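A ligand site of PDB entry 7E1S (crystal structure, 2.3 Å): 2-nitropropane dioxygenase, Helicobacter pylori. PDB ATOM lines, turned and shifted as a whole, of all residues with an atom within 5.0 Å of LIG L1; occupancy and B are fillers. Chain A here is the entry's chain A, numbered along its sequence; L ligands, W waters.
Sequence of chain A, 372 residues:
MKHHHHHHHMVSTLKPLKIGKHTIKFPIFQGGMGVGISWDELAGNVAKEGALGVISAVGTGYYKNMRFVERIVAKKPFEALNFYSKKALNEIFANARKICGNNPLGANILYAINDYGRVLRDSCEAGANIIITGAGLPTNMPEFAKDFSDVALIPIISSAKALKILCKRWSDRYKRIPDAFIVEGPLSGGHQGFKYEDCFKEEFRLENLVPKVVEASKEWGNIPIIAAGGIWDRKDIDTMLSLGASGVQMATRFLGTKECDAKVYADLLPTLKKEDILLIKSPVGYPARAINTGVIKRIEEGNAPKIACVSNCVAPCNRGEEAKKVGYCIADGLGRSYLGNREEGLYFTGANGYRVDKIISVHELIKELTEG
The side-chain carboxylate (OE2) of Glu 184 lies within hydrogen-bond range of an oxygen (O4) of LIG L1.
The backbone NH (N) of Thr 252 lies within hydrogen-bond range of an oxygen (O8) of LIG L1 (3.0 Å).
The side-chain hydroxyl (OG1) of Thr 252 sits at hydrogen-bond distance from an oxygen (O8) of LIG L1 (2.7 Å).
The backbone NH (N) of Gly 230 sits at hydrogen-bond distance from an oxygen (O9) of LIG L1, 2.7 Å away.
The backbone NH (N) of Gly 32 lies within hydrogen-bond range of an oxygen (O3) of LIG L1.
The backbone carbonyl oxygen (O) of Gly 32 is in hydrogen-bond range of an oxygen (O3) of LIG L1 (2.8 Å).
N of Ala 251 is in hydrogen-bond range of O7 of LIG L1.
The side-chain amide oxygen of Asn 108 lies within hydrogen-bond range of a nitrogen (N2) of LIG L1 (2.9 Å).
The side-chain amide nitrogen of Gln 249 lies within hydrogen-bond range of an oxygen (O4) of LIG L1 (3.0 Å).
N of Gly 189 sits at hydrogen-bond distance from O5 of LIG L1 (3.2 Å).
The backbone NH (N) of Gly 229 lies close to an oxygen (O6) of LIG L1, at 3.4 Å.
The backbone NH (N) of Gly 34 sits at hydrogen-bond distance from an oxygen (O2) of LIG L1 (3.4 Å).
OE1 of Glu 184 is in hydrogen-bond range of N2 of LG2 L2, at 2.9 Å.
Residues that only touch LIG L1: Gly 31, Met 33, Ile 37, Leu 110, Ile 156, Leu 187, Ser 188, Gly 190, Met 250, Phe 348, Thr 349 and Gly 350.
Hydrophobic or aromatic side chains that line LIG L1: Met 33, Ile 37, Leu 110, Ile 156, Ala 251 and Phe 348.
Within 4 Å of LIG L1: Gly 31, Gly 32, Met 33, Gly 34, Ile 37, Asn 108, Leu 110, Ile 156, Glu 184, Leu 187, Ser 188, Gly 189, Gly 190, Gly 229, Gly 230, Gln 249, Met 250, Ala 251, Thr 252, Phe 348, Thr 349 and Gly 350.
The nearest printed residue that does not touch LIG L1 is Ala 228 (4.1 Å).
The side-chain carboxylate (OE1) of Glu 184 lies close to the side-chain hydroxyl (OG) of Ser 188 (3.5 Å).
The backbone NH (N) of Gly 350 sits at hydrogen-bond distance from the side-chain hydroxyl (OG1) of Thr 252 (3.0 Å).
The backbone carbonyl oxygen of Gly 230 lies within hydrogen-bond range of the side-chain amide nitrogen of Asn 352.
The backbone carbonyl oxygen (O) of Met 250 sits at hydrogen-bond distance from the backbone NH (N) of Gly 31, 2.8 Å away.
The side-chain hydroxyl of Tyr 265 sits at hydrogen-bond distance from the backbone NH of Phe 348, at 3.1 Å.
N2 of LIG L1 lies close to S1 of LG2 L2 (3.6 Å).
Water W2 lies within hydrogen-bond range of O7 of LIG L1 (2.5 Å), O of Ile 231 (2.9 Å) and N of Thr 252 (3.4 Å).
Water W4 lies within hydrogen-bond range of O7 of LIG L1 (2.6 Å), O of Gln 249 (2.8 Å), N of Gly 229 (3.1 Å) and N of Ile 231 (3.1 Å).
Water W6 lies within hydrogen-bond range of OG of Ser 56, O2 of LIG L1 and OD1 of Asn 108.
Water W3 lies within hydrogen-bond range of O9 of LIG L1 (2.7 Å), O of Leu 187 (2.9 Å) and N of Asn 352 (2.9 Å).
Water W5 lies within hydrogen-bond range of the side-chain amide nitrogen (ND2) of Asn 352, an oxygen (O9) of LIG L1 and the backbone carbonyl oxygen (O) of Ile 231.
Water W1 lies within hydrogen-bond range of OD1 of Asn 108 (2.8 Å), N of Gly 134 (2.9 Å), O1 of LIG L1 (3.1 Å) and N of Leu 110 (3.4 Å).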
ATOM      1  N   GLY A  31       2.110 -33.492  11.089  1.00  0.00           N
ATOM      2  CA  GLY A  31       2.612 -32.199  11.526  1.00  0.00           C
ATOM      3  C   GLY A  31       3.158 -32.241  12.947  1.00  0.00           C
ATOM      4  O   GLY A  31       2.646 -32.948  13.816  1.00  0.00           O
ATOM      5  N   GLY A  32       4.219 -31.475  13.159  1.00  0.00           N
ATOM      6  CA  GLY A  32       4.792 -31.385  14.481  1.00  0.00           C
ATOM      7  C   GLY A  32       3.888 -30.630  15.445  1.00  0.00           C
ATOM      8  O   GLY A  32       3.143 -29.730  15.056  1.00  0.00           O
ATOM      9  N   MET A  33       3.957 -31.033  16.712  1.00  0.00           N
ATOM     10  CA  MET A  33       2.993 -30.552  17.721  1.00  0.00           C
ATOM     11  C   MET A  33       3.701 -30.483  19.069  1.00  0.00           C
ATOM     12  O   MET A  33       4.073 -31.516  19.638  1.00  0.00           O
ATOM     13  CB  MET A  33       1.769 -31.480  17.785  1.00  0.00           C
ATOM     14  CG  MET A  33       0.692 -31.211  16.728  1.00  0.00           C
ATOM     15  SD  MET A  33      -0.689 -32.389  16.607  1.00  0.00           S
ATOM     16  CE  MET A  33       0.135 -33.966  16.414  1.00  0.00           C
ATOM     17  N   GLY A  34       3.897 -29.267  19.594  1.00  0.00           N
ATOM     18  CA  GLY A  34       4.498 -29.096  20.913  1.00  0.00           C
ATOM     19  C   GLY A  34       3.445 -28.676  21.924  1.00  0.00           C
ATOM     20  O   GLY A  34       2.392 -28.171  21.521  1.00  0.00           O
ATOM     21  N   ILE A  37       3.646 -33.442  22.330  1.00  0.00           N
ATOM     22  CA  ILE A  37       2.524 -34.065  21.639  1.00  0.00           C
ATOM     23  C   ILE A  37       3.005 -35.042  20.566  1.00  0.00           C
ATOM     24  O   ILE A  37       2.592 -36.207  20.541  1.00  0.00           O
ATOM     25  CB  ILE A  37       1.586 -32.978  21.040  1.00  0.00           C
ATOM     26  CG1 ILE A  37       1.022 -32.083  22.161  1.00  0.00           C
ATOM     27  CG2 ILE A  37       0.458 -33.625  20.239  1.00  0.00           C
ATOM     28  CD1 ILE A  37       0.047 -30.998  21.675  1.00  0.00           C
ATOM     29  N   SER A  56       8.541 -32.850  17.414  1.00  0.00           N
ATOM     30  CA  SER A  56       8.664 -31.471  17.878  1.00  0.00           C
ATOM     31  C   SER A  56       9.815 -31.383  18.869  1.00  0.00           C
ATOM     32  O   SER A  56       9.950 -32.224  19.758  1.00  0.00           O
ATOM     33  CB  SER A  56       7.369 -30.987  18.517  1.00  0.00           C
ATOM     34  OG  SER A  56       7.589 -29.779  19.226  1.00  0.00           O
ATOM     35  N   VAL A  58      10.458 -28.490  20.690  1.00  0.00           N
ATOM     36  CA  VAL A  58      10.216 -27.366  21.603  1.00  0.00           C
ATOM     37  C   VAL A  58       9.754 -27.896  22.963  1.00  0.00           C
ATOM     38  O   VAL A  58       8.877 -28.765  23.058  1.00  0.00           O
ATOM     39  CB  VAL A  58       9.185 -26.385  21.002  1.00  0.00           C
ATOM     40  CG1 VAL A  58       9.698 -25.864  19.650  1.00  0.00           C
ATOM     41  CG2 VAL A  58       7.812 -27.019  20.862  1.00  0.00           C
ATOM     42  N   ASN A 108      10.688 -30.474  14.204  1.00  0.00           N
ATOM     43  CA  ASN A 108       9.981 -29.211  14.071  1.00  0.00           C
ATOM     44  C   ASN A 108      10.508 -28.202  15.104  1.00  0.00           C
ATOM     45  O   ASN A 108      10.647 -28.514  16.294  1.00  0.00           O
ATOM     46  CB  ASN A 108       8.464 -29.421  14.198  1.00  0.00           C
ATOM     47  CG  ASN A 108       7.653 -28.143  13.887  1.00  0.00           C
ATOM     48  OD1 ASN A 108       7.717 -27.155  14.624  1.00  0.00           O
ATOM     49  ND2 ASN A 108       6.881 -28.192  12.815  1.00  0.00           N
ATOM     50  N   LEU A 110      10.148 -24.014  15.973  1.00  0.00           N
ATOM     51  CA  LEU A 110       9.713 -22.653  15.702  1.00  0.00           C
ATOM     52  C   LEU A 110      10.932 -21.733  15.598  1.00  0.00           C
ATOM     53  O   LEU A 110      11.846 -21.806  16.419  1.00  0.00           O
ATOM     54  CB  LEU A 110       8.800 -22.171  16.818  1.00  0.00           C
ATOM     55  CG  LEU A 110       7.351 -22.634  16.864  1.00  0.00           C
ATOM     56  CD1 LEU A 110       7.247 -24.123  17.218  1.00  0.00           C
ATOM     57  CD2 LEU A 110       6.652 -21.792  17.921  1.00  0.00           C
ATOM     58  N   GLY A 134       8.553 -23.060  11.228  1.00  0.00           N
ATOM     59  CA  GLY A 134       7.636 -21.951  11.067  1.00  0.00           C
ATOM     60  C   GLY A 134       7.781 -20.909  12.167  1.00  0.00           C
ATOM     61  O   GLY A 134       8.878 -20.749  12.727  1.00  0.00           O
ATOM     62  N   ILE A 156       7.839 -23.255   6.791  1.00  0.00           N
ATOM     63  CA  ILE A 156       6.387 -23.139   6.738  1.00  0.00           C
ATOM     64  C   ILE A 156       6.082 -21.705   6.374  1.00  0.00           C
ATOM     65  O   ILE A 156       6.661 -20.771   6.942  1.00  0.00           O
ATOM     66  CB  ILE A 156       5.736 -23.516   8.085  1.00  0.00           C
ATOM     67  CG1 ILE A 156       6.264 -24.858   8.563  1.00  0.00           C
ATOM     68  CG2 ILE A 156       4.258 -23.554   7.904  1.00  0.00           C
ATOM     69  CD1 ILE A 156       5.961 -25.152   9.982  1.00  0.00           C
ATOM     70  N   GLU A 184       0.595 -23.342   5.075  1.00  0.00           N
ATOM     71  CA  GLU A 184      -0.318 -23.565   6.183  1.00  0.00           C
ATOM     72  C   GLU A 184      -1.471 -22.573   6.117  1.00  0.00           C
ATOM     73  O   GLU A 184      -1.263 -21.363   6.185  1.00  0.00           O
ATOM     74  CB  GLU A 184       0.367 -23.452   7.549  1.00  0.00           C
ATOM     75  CG  GLU A 184      -0.487 -24.121   8.628  1.00  0.00           C
ATOM     76  CD  GLU A 184       0.133 -24.062  10.012  1.00  0.00           C
ATOM     77  OE1 GLU A 184       0.514 -22.957  10.451  1.00  0.00           O
ATOM     78  OE2 GLU A 184       0.236 -25.133  10.648  1.00  0.00           O
ATOM     79  N   LEU A 187      -7.139 -22.858   8.790  1.00  0.00           N
ATOM     80  CA  LEU A 187      -7.861 -23.872   9.566  1.00  0.00           C
ATOM     81  C   LEU A 187      -6.945 -24.694  10.462  1.00  0.00           C
ATOM     82  O   LEU A 187      -7.398 -25.671  11.061  1.00  0.00           O
ATOM     83  CB  LEU A 187      -8.640 -24.804   8.643  1.00  0.00           C
ATOM     84  CG  LEU A 187      -9.718 -24.160   7.769  1.00  0.00           C
ATOM     85  CD1 LEU A 187     -10.359 -25.214   6.855  1.00  0.00           C
ATOM     86  CD2 LEU A 187     -10.762 -23.436   8.622  1.00  0.00           C
ATOM     87  N   SER A 188      -5.662 -24.291  10.579  1.00  0.00           N
ATOM     88  CA  SER A 188      -4.667 -25.113  11.237  1.00  0.00           C
ATOM     89  C   SER A 188      -4.750 -24.979  12.752  1.00  0.00           C
ATOM     90  O   SER A 188      -5.422 -24.093  13.290  1.00  0.00           O
ATOM     91  CB  SER A 188      -3.260 -24.751  10.733  1.00  0.00           C
ATOM     92  OG  SER A 188      -2.842 -23.481  11.206  1.00  0.00           O
ATOM     93  N   GLY A 189      -4.067 -25.888  13.440  1.00  0.00           N
ATOM     94  CA  GLY A 189      -3.915 -25.783  14.874  1.00  0.00           C
ATOM     95  C   GLY A 189      -2.711 -24.933  15.248  1.00  0.00           C
ATOM     96  O   GLY A 189      -1.872 -24.612  14.415  1.00  0.00           O
ATOM     97  N   GLY A 190      -2.636 -24.549  16.525  1.00  0.00           N
ATOM     98  CA  GLY A 190      -1.507 -23.748  16.969  1.00  0.00           C
ATOM     99  C   GLY A 190      -1.536 -22.363  16.332  1.00  0.00           C
ATOM    100  O   GLY A 190      -2.595 -21.800  16.049  1.00  0.00           O
ATOM    101  N   ALA A 228      -1.268 -27.748   4.199  1.00  0.00           N
ATOM    102  CA  ALA A 228      -1.613 -28.054   5.580  1.00  0.00           C
ATOM    103  C   ALA A 228      -2.656 -27.060   6.051  1.00  0.00           C
ATOM    104  O   ALA A 228      -2.675 -25.891   5.638  1.00  0.00           O
ATOM    105  CB  ALA A 228      -0.380 -28.024   6.491  1.00  0.00           C
ATOM    106  N   GLY A 229      -3.526 -27.543   6.936  1.00  0.00           N
ATOM    107  CA  GLY A 229      -4.563 -26.722   7.531  1.00  0.00           C
ATOM    108  C   GLY A 229      -5.965 -27.122   7.151  1.00  0.00           C
ATOM    109  O   GLY A 229      -6.476 -26.680   6.118  1.00  0.00           O
ATOM    110  N   GLY A 230      -6.625 -27.936   7.970  1.00  0.00           N
ATOM    111  CA  GLY A 230      -7.982 -28.352   7.667  1.00  0.00           C
ATOM    112  C   GLY A 230      -8.130 -29.570   6.773  1.00  0.00           C
ATOM    113  O   GLY A 230      -9.250 -29.891   6.370  1.00  0.00           O
ATOM    114  N   ILE A 231      -7.041 -30.258   6.455  1.00  0.00           N
ATOM    115  CA  ILE A 231      -7.118 -31.478   5.643  1.00  0.00           C
ATOM    116  C   ILE A 231      -7.551 -32.624   6.540  1.00  0.00           C
ATOM    117  O   ILE A 231      -6.852 -32.970   7.492  1.00  0.00           O
ATOM    118  CB  ILE A 231      -5.770 -31.749   4.960  1.00  0.00           C
ATOM    119  CG1 ILE A 231      -5.406 -30.585   4.050  1.00  0.00           C
ATOM    120  CG2 ILE A 231      -5.789 -32.997   4.144  1.00  0.00           C
ATOM    121  CD1 ILE A 231      -3.957 -30.585   3.620  1.00  0.00           C
ATOM    122  N   GLN A 249       0.407 -32.029   4.845  1.00  0.00           N
ATOM    123  CA  GLN A 249       0.739 -32.161   6.254  1.00  0.00           C
ATOM    124  C   GLN A 249      -0.554 -32.131   7.048  1.00  0.00           C
ATOM    125  O   GLN A 249      -1.438 -31.314   6.770  1.00  0.00           O
ATOM    126  CB  GLN A 249       1.671 -31.026   6.734  1.00  0.00           C
ATOM    127  CG  GLN A 249       1.923 -31.062   8.222  1.00  0.00           C
ATOM    128  CD  GLN A 249       3.109 -30.216   8.683  1.00  0.00           C
ATOM    129  OE1 GLN A 249       4.251 -30.676   8.703  1.00  0.00           O
ATOM    130  NE2 GLN A 249       2.827 -28.973   9.069  1.00  0.00           N
ATOM    131  N   MET A 250      -0.677 -33.029   8.027  1.00  0.00           N
ATOM    132  CA  MET A 250      -1.900 -33.178   8.797  1.00  0.00           C
ATOM    133  C   MET A 250      -1.535 -33.337  10.268  1.00  0.00           C
ATOM    134  O   MET A 250      -0.610 -34.091  10.600  1.00  0.00           O
ATOM    135  CB  MET A 250      -2.715 -34.398   8.334  1.00  0.00           C
ATOM    136  CG  MET A 250      -3.405 -34.226   6.991  1.00  0.00           C
ATOM    137  SD  MET A 250      -4.027 -35.811   6.320  1.00  0.00           S
ATOM    138  CE  MET A 250      -5.519 -35.968   7.278  1.00  0.00           C
ATOM    139  N   ALA A 251      -2.246 -32.638  11.156  1.00  0.00           N
ATOM    140  CA  ALA A 251      -1.941 -32.733  12.577  1.00  0.00           C
ATOM    141  C   ALA A 251      -3.128 -33.158  13.426  1.00  0.00           C
ATOM    142  O   ALA A 251      -2.959 -34.004  14.307  1.00  0.00           O
ATOM    143  CB  ALA A 251      -1.399 -31.399  13.121  1.00  0.00           C
ATOM    144  N   THR A 252      -4.314 -32.565  13.210  1.00  0.00           N
ATOM    145  CA  THR A 252      -5.449 -32.828  14.109  1.00  0.00           C
ATOM    146  C   THR A 252      -5.859 -34.301  14.097  1.00  0.00           C
ATOM    147  O   THR A 252      -6.157 -34.852  15.156  1.00  0.00           O
ATOM    148  CB  THR A 252      -6.636 -31.919  13.759  1.00  0.00           C
ATOM    149  OG1 THR A 252      -6.321 -30.553  14.064  1.00  0.00           O
ATOM    150  CG2 THR A 252      -7.885 -32.347  14.566  1.00  0.00           C
ATOM    151  N   LEU A 255      -3.469 -35.949  16.143  1.00  0.00           N
ATOM    152  CA  LEU A 255      -3.704 -35.549  17.535  1.00  0.00           C
ATOM    153  C   LEU A 255      -4.706 -36.481  18.185  1.00  0.00           C
ATOM    154  O   LEU A 255      -4.583 -36.766  19.381  1.00  0.00           O
ATOM    155  CB  LEU A 255      -4.170 -34.086  17.606  1.00  0.00           C
ATOM    156  CG  LEU A 255      -4.365 -33.410  18.977  1.00  0.00           C
ATOM    157  CD1 LEU A 255      -3.076 -33.335  19.796  1.00  0.00           C
ATOM    158  CD2 LEU A 255      -5.057 -32.040  18.880  1.00  0.00           C
ATOM    159  N   TYR A 265      -4.976 -35.769  25.485  1.00  0.00           N
ATOM    160  CA  TYR A 265      -5.800 -35.451  24.316  1.00  0.00           C
ATOM    161  C   TYR A 265      -6.782 -36.555  23.961  1.00  0.00           C
ATOM    162  O   TYR A 265      -7.782 -36.263  23.315  1.00  0.00           O
ATOM    163  CB  TYR A 265      -4.914 -35.133  23.097  1.00  0.00           C
ATOM    164  CG  TYR A 265      -4.456 -33.691  23.060  1.00  0.00           C
ATOM    165  CD1 TYR A 265      -5.273 -32.694  22.542  1.00  0.00           C
ATOM    166  CD2 TYR A 265      -3.212 -33.313  23.563  1.00  0.00           C
ATOM    167  CE1 TYR A 265      -4.859 -31.345  22.533  1.00  0.00           C
ATOM    168  CE2 TYR A 265      -2.803 -32.010  23.550  1.00  0.00           C
ATOM    169  CZ  TYR A 265      -3.616 -31.026  23.031  1.00  0.00           C
ATOM    170  OH  TYR A 265      -3.169 -29.719  23.033  1.00  0.00           O
ATOM    171  N   PHE A 348      -4.331 -26.977  22.315  1.00  0.00           N
ATOM    172  CA  PHE A 348      -4.521 -26.512  20.957  1.00  0.00           C
ATOM    173  C   PHE A 348      -5.294 -27.537  20.151  1.00  0.00           C
ATOM    174  O   PHE A 348      -5.464 -28.699  20.566  1.00  0.00           O
ATOM    175  CB  PHE A 348      -3.171 -26.210  20.290  1.00  0.00           C
ATOM    176  CG  PHE A 348      -2.533 -24.907  20.747  1.00  0.00           C
ATOM    177  CD1 PHE A 348      -3.253 -23.976  21.479  1.00  0.00           C
ATOM    178  CD2 PHE A 348      -1.217 -24.629  20.424  1.00  0.00           C
ATOM    179  CE1 PHE A 348      -2.666 -22.776  21.907  1.00  0.00           C
ATOM    180  CE2 PHE A 348      -0.614 -23.424  20.840  1.00  0.00           C
ATOM    181  CZ  PHE A 348      -1.338 -22.509  21.578  1.00  0.00           C
ATOM    182  N   THR A 349      -5.758 -27.104  18.982  1.00  0.00           N
ATOM    183  CA  THR A 349      -6.414 -27.979  18.031  1.00  0.00           C
ATOM    184  C   THR A 349      -6.544 -27.233  16.709  1.00  0.00           C
ATOM    185  O   THR A 349      -6.574 -26.008  16.678  1.00  0.00           O
ATOM    186  CB  THR A 349      -7.808 -28.426  18.507  1.00  0.00           C
ATOM    187  OG1 THR A 349      -8.425 -29.254  17.506  1.00  0.00           O
ATOM    188  CG2 THR A 349      -8.705 -27.222  18.714  1.00  0.00           C
ATOM    189  N   GLY A 350      -6.665 -27.989  15.635  1.00  0.00           N
ATOM    190  CA  GLY A 350      -7.117 -27.405  14.404  1.00  0.00           C
ATOM    191  C   GLY A 350      -8.619 -27.193  14.433  1.00  0.00           C
ATOM    192  O   GLY A 350      -9.335 -27.670  15.313  1.00  0.00           O
ATOM    193  N   ASN A 352     -10.819 -28.538  12.789  1.00  0.00           N
ATOM    194  CA  ASN A 352     -11.549 -29.792  12.616  1.00  0.00           C
ATOM    195  C   ASN A 352     -11.554 -30.671  13.863  1.00  0.00           C
ATOM    196  O   ASN A 352     -12.074 -31.793  13.805  1.00  0.00           O
ATOM    197  CB  ASN A 352     -10.945 -30.602  11.443  1.00  0.00           C
ATOM    198  CG  ASN A 352     -11.459 -30.169  10.076  1.00  0.00           C
ATOM    199  OD1 ASN A 352     -12.604 -29.747   9.930  1.00  0.00           O
ATOM    200  ND2 ASN A 352     -10.618 -30.303   9.050  1.00  0.00           N
HETATM  201  N1  LIG L   1       3.068 -26.340  13.868  1.00  0.00           N
HETATM  202  C1  LIG L   1       4.429 -26.099  14.024  1.00  0.00           C
HETATM  203  O1  LIG L   1       5.096 -25.753  13.046  1.00  0.00           O
HETATM  204  N2  LIG L   1       5.024 -26.275  15.287  1.00  0.00           N
HETATM  205  C2  LIG L   1       4.238 -26.683  16.373  1.00  0.00           C
HETATM  206  O2  LIG L   1       4.772 -26.825  17.466  1.00  0.00           O
HETATM  207  C3  LIG L   1       2.871 -26.918  16.211  1.00  0.00           C
HETATM  208  N3  LIG L   1       2.123 -27.308  17.253  1.00  0.00           N
HETATM  209  C4  LIG L   1       0.848 -27.694  17.071  1.00  0.00           C
HETATM  210  C5  LIG L   1       0.122 -28.261  18.145  1.00  0.00           C
HETATM  211  C6  LIG L   1      -1.186 -28.707  17.938  1.00  0.00           C
HETATM  212  C7  LIG L   1      -1.927 -29.279  19.006  1.00  0.00           C
HETATM  213  C8  LIG L   1      -1.751 -28.582  16.662  1.00  0.00           C
HETATM  214  C9  LIG L   1      -3.062 -29.007  16.425  1.00  0.00           C
HETATM  215  C10 LIG L   1      -1.034 -28.024  15.607  1.00  0.00           C
HETATM  216  C11 LIG L   1       0.261 -27.567  15.803  1.00  0.00           C
HETATM  217  N4  LIG L   1       0.986 -27.044  14.777  1.00  0.00           N
HETATM  218  C12 LIG L   1       2.281 -26.755  14.965  1.00  0.00           C
HETATM  219  C13 LIG L   1       0.445 -26.992  13.396  1.00  0.00           C
HETATM  220  C14 LIG L   1       0.496 -28.404  12.718  1.00  0.00           C
HETATM  221  O3  LIG L   1       1.845 -28.952  12.684  1.00  0.00           O
HETATM  222  C15 LIG L   1      -0.110 -28.400  11.309  1.00  0.00           C
HETATM  223  O4  LIG L   1       0.622 -27.522  10.437  1.00  0.00           O
HETATM  224  C16 LIG L   1      -1.610 -28.026  11.283  1.00  0.00           C
HETATM  225  O5  LIG L   1      -2.253 -28.342  12.518  1.00  0.00           O
HETATM  226  C17 LIG L   1      -2.278 -28.810  10.127  1.00  0.00           C
HETATM  227  O6  LIG L   1      -3.675 -28.612  10.150  1.00  0.00           O
HETATM  228  P1  LIG L   1      -4.690 -29.731  10.770  1.00  0.00           P
HETATM  229  O7  LIG L   1      -4.295 -30.959  10.051  1.00  0.00           O
HETATM  230  O8  LIG L   1      -4.444 -29.777  12.218  1.00  0.00           O
HETATM  231  O9  LIG L   1      -5.971 -29.165  10.341  1.00  0.00           O
HETATM  232  P1  LG2 L   2       6.402 -12.179  11.011  1.00  0.00           P
HETATM  233  O1  LG2 L   2       5.498 -11.307  11.416  1.00  0.00           O
HETATM  234  O2  LG2 L   2       7.076 -12.833  12.117  1.00  0.00           O
HETATM  235  O3  LG2 L   2       5.670 -12.892   9.946  1.00  0.00           O
HETATM  236  C1  LG2 L   2       5.942 -14.249   9.621  1.00  0.00           C
HETATM  237  C2  LG2 L   2       4.910 -15.220   9.110  1.00  0.00           C
HETATM  238  C3  LG2 L   2       4.220 -14.388   8.151  1.00  0.00           C
HETATM  239  C4  LG2 L   2       3.965 -15.680  10.197  1.00  0.00           C
HETATM  240  C5  LG2 L   2       5.486 -16.464   8.407  1.00  0.00           C
HETATM  241  O4  LG2 L   2       6.486 -17.159   9.079  1.00  0.00           O
HETATM  242  C6  LG2 L   2       4.547 -17.461   7.745  1.00  0.00           C
HETATM  243  O5  LG2 L   2       4.064 -17.305   6.700  1.00  0.00           O
HETATM  244  N1  LG2 L   2       4.321 -18.463   8.445  1.00  0.00           N
HETATM  245  C7  LG2 L   2       3.674 -19.700   8.578  1.00  0.00           C
HETATM  246  C8  LG2 L   2       4.205 -20.290   9.931  1.00  0.00           C
HETATM  247  C9  LG2 L   2       3.139 -21.108  10.496  1.00  0.00           C
HETATM  248  O6  LG2 L   2       2.091 -20.858  10.063  1.00  0.00           O
HETATM  249  N2  LG2 L   2       3.107 -22.047  11.347  1.00  0.00           N
HETATM  250  C10 LG2 L   2       3.999 -22.707  12.125  1.00  0.00           C
HETATM  251  C11 LG2 L   2       3.719 -22.099  13.469  1.00  0.00           C
HETATM  252  S1  LG2 L   2       4.468 -22.768  14.878  1.00  0.00           S
HETATM  253  C12 LG2 L   2       2.966 -23.237  15.565  1.00  0.00           C
HETATM  254  O7  LG2 L   2       1.990 -23.386  15.009  1.00  0.00           O
HETATM  255  C13 LG2 L   2       2.567 -23.558  16.957  1.00  0.00           C
HETATM  256  C14 LG2 L   2       3.600 -23.826  17.901  1.00  0.00           C
HETATM  257  C15 LG2 L   2       2.890 -24.535  18.993  1.00  0.00           C
HETATM  258  C16 LG2 L   2       3.947 -24.642  20.094  1.00  0.00           C
HETATM  259  C17 LG2 L   2       4.550 -23.407  20.740  1.00  0.00           C
HETATM  260  C18 LG2 L   2       5.762 -23.875  21.513  1.00  0.00           C
HETATM  261  C19 LG2 L   2       6.466 -23.008  22.548  1.00  0.00           C
HETATM  262  O   HOH W   1       7.892 -24.583  13.557  1.00  0.00           O
HETATM  263  O   HOH W   2      -5.560 -33.125  10.106  1.00  0.00           O
HETATM  264  O   HOH W   3      -8.491 -28.384  11.000  1.00  0.00           O
HETATM  265  O   HOH W   4      -4.092 -30.548   7.456  1.00  0.00           O
HETATM  266  O   HOH W   5      -8.018 -31.265   9.728  1.00  0.00           O
HETATM  267  O   HOH W   6       7.251 -27.865  17.615  1.00  0.00           O
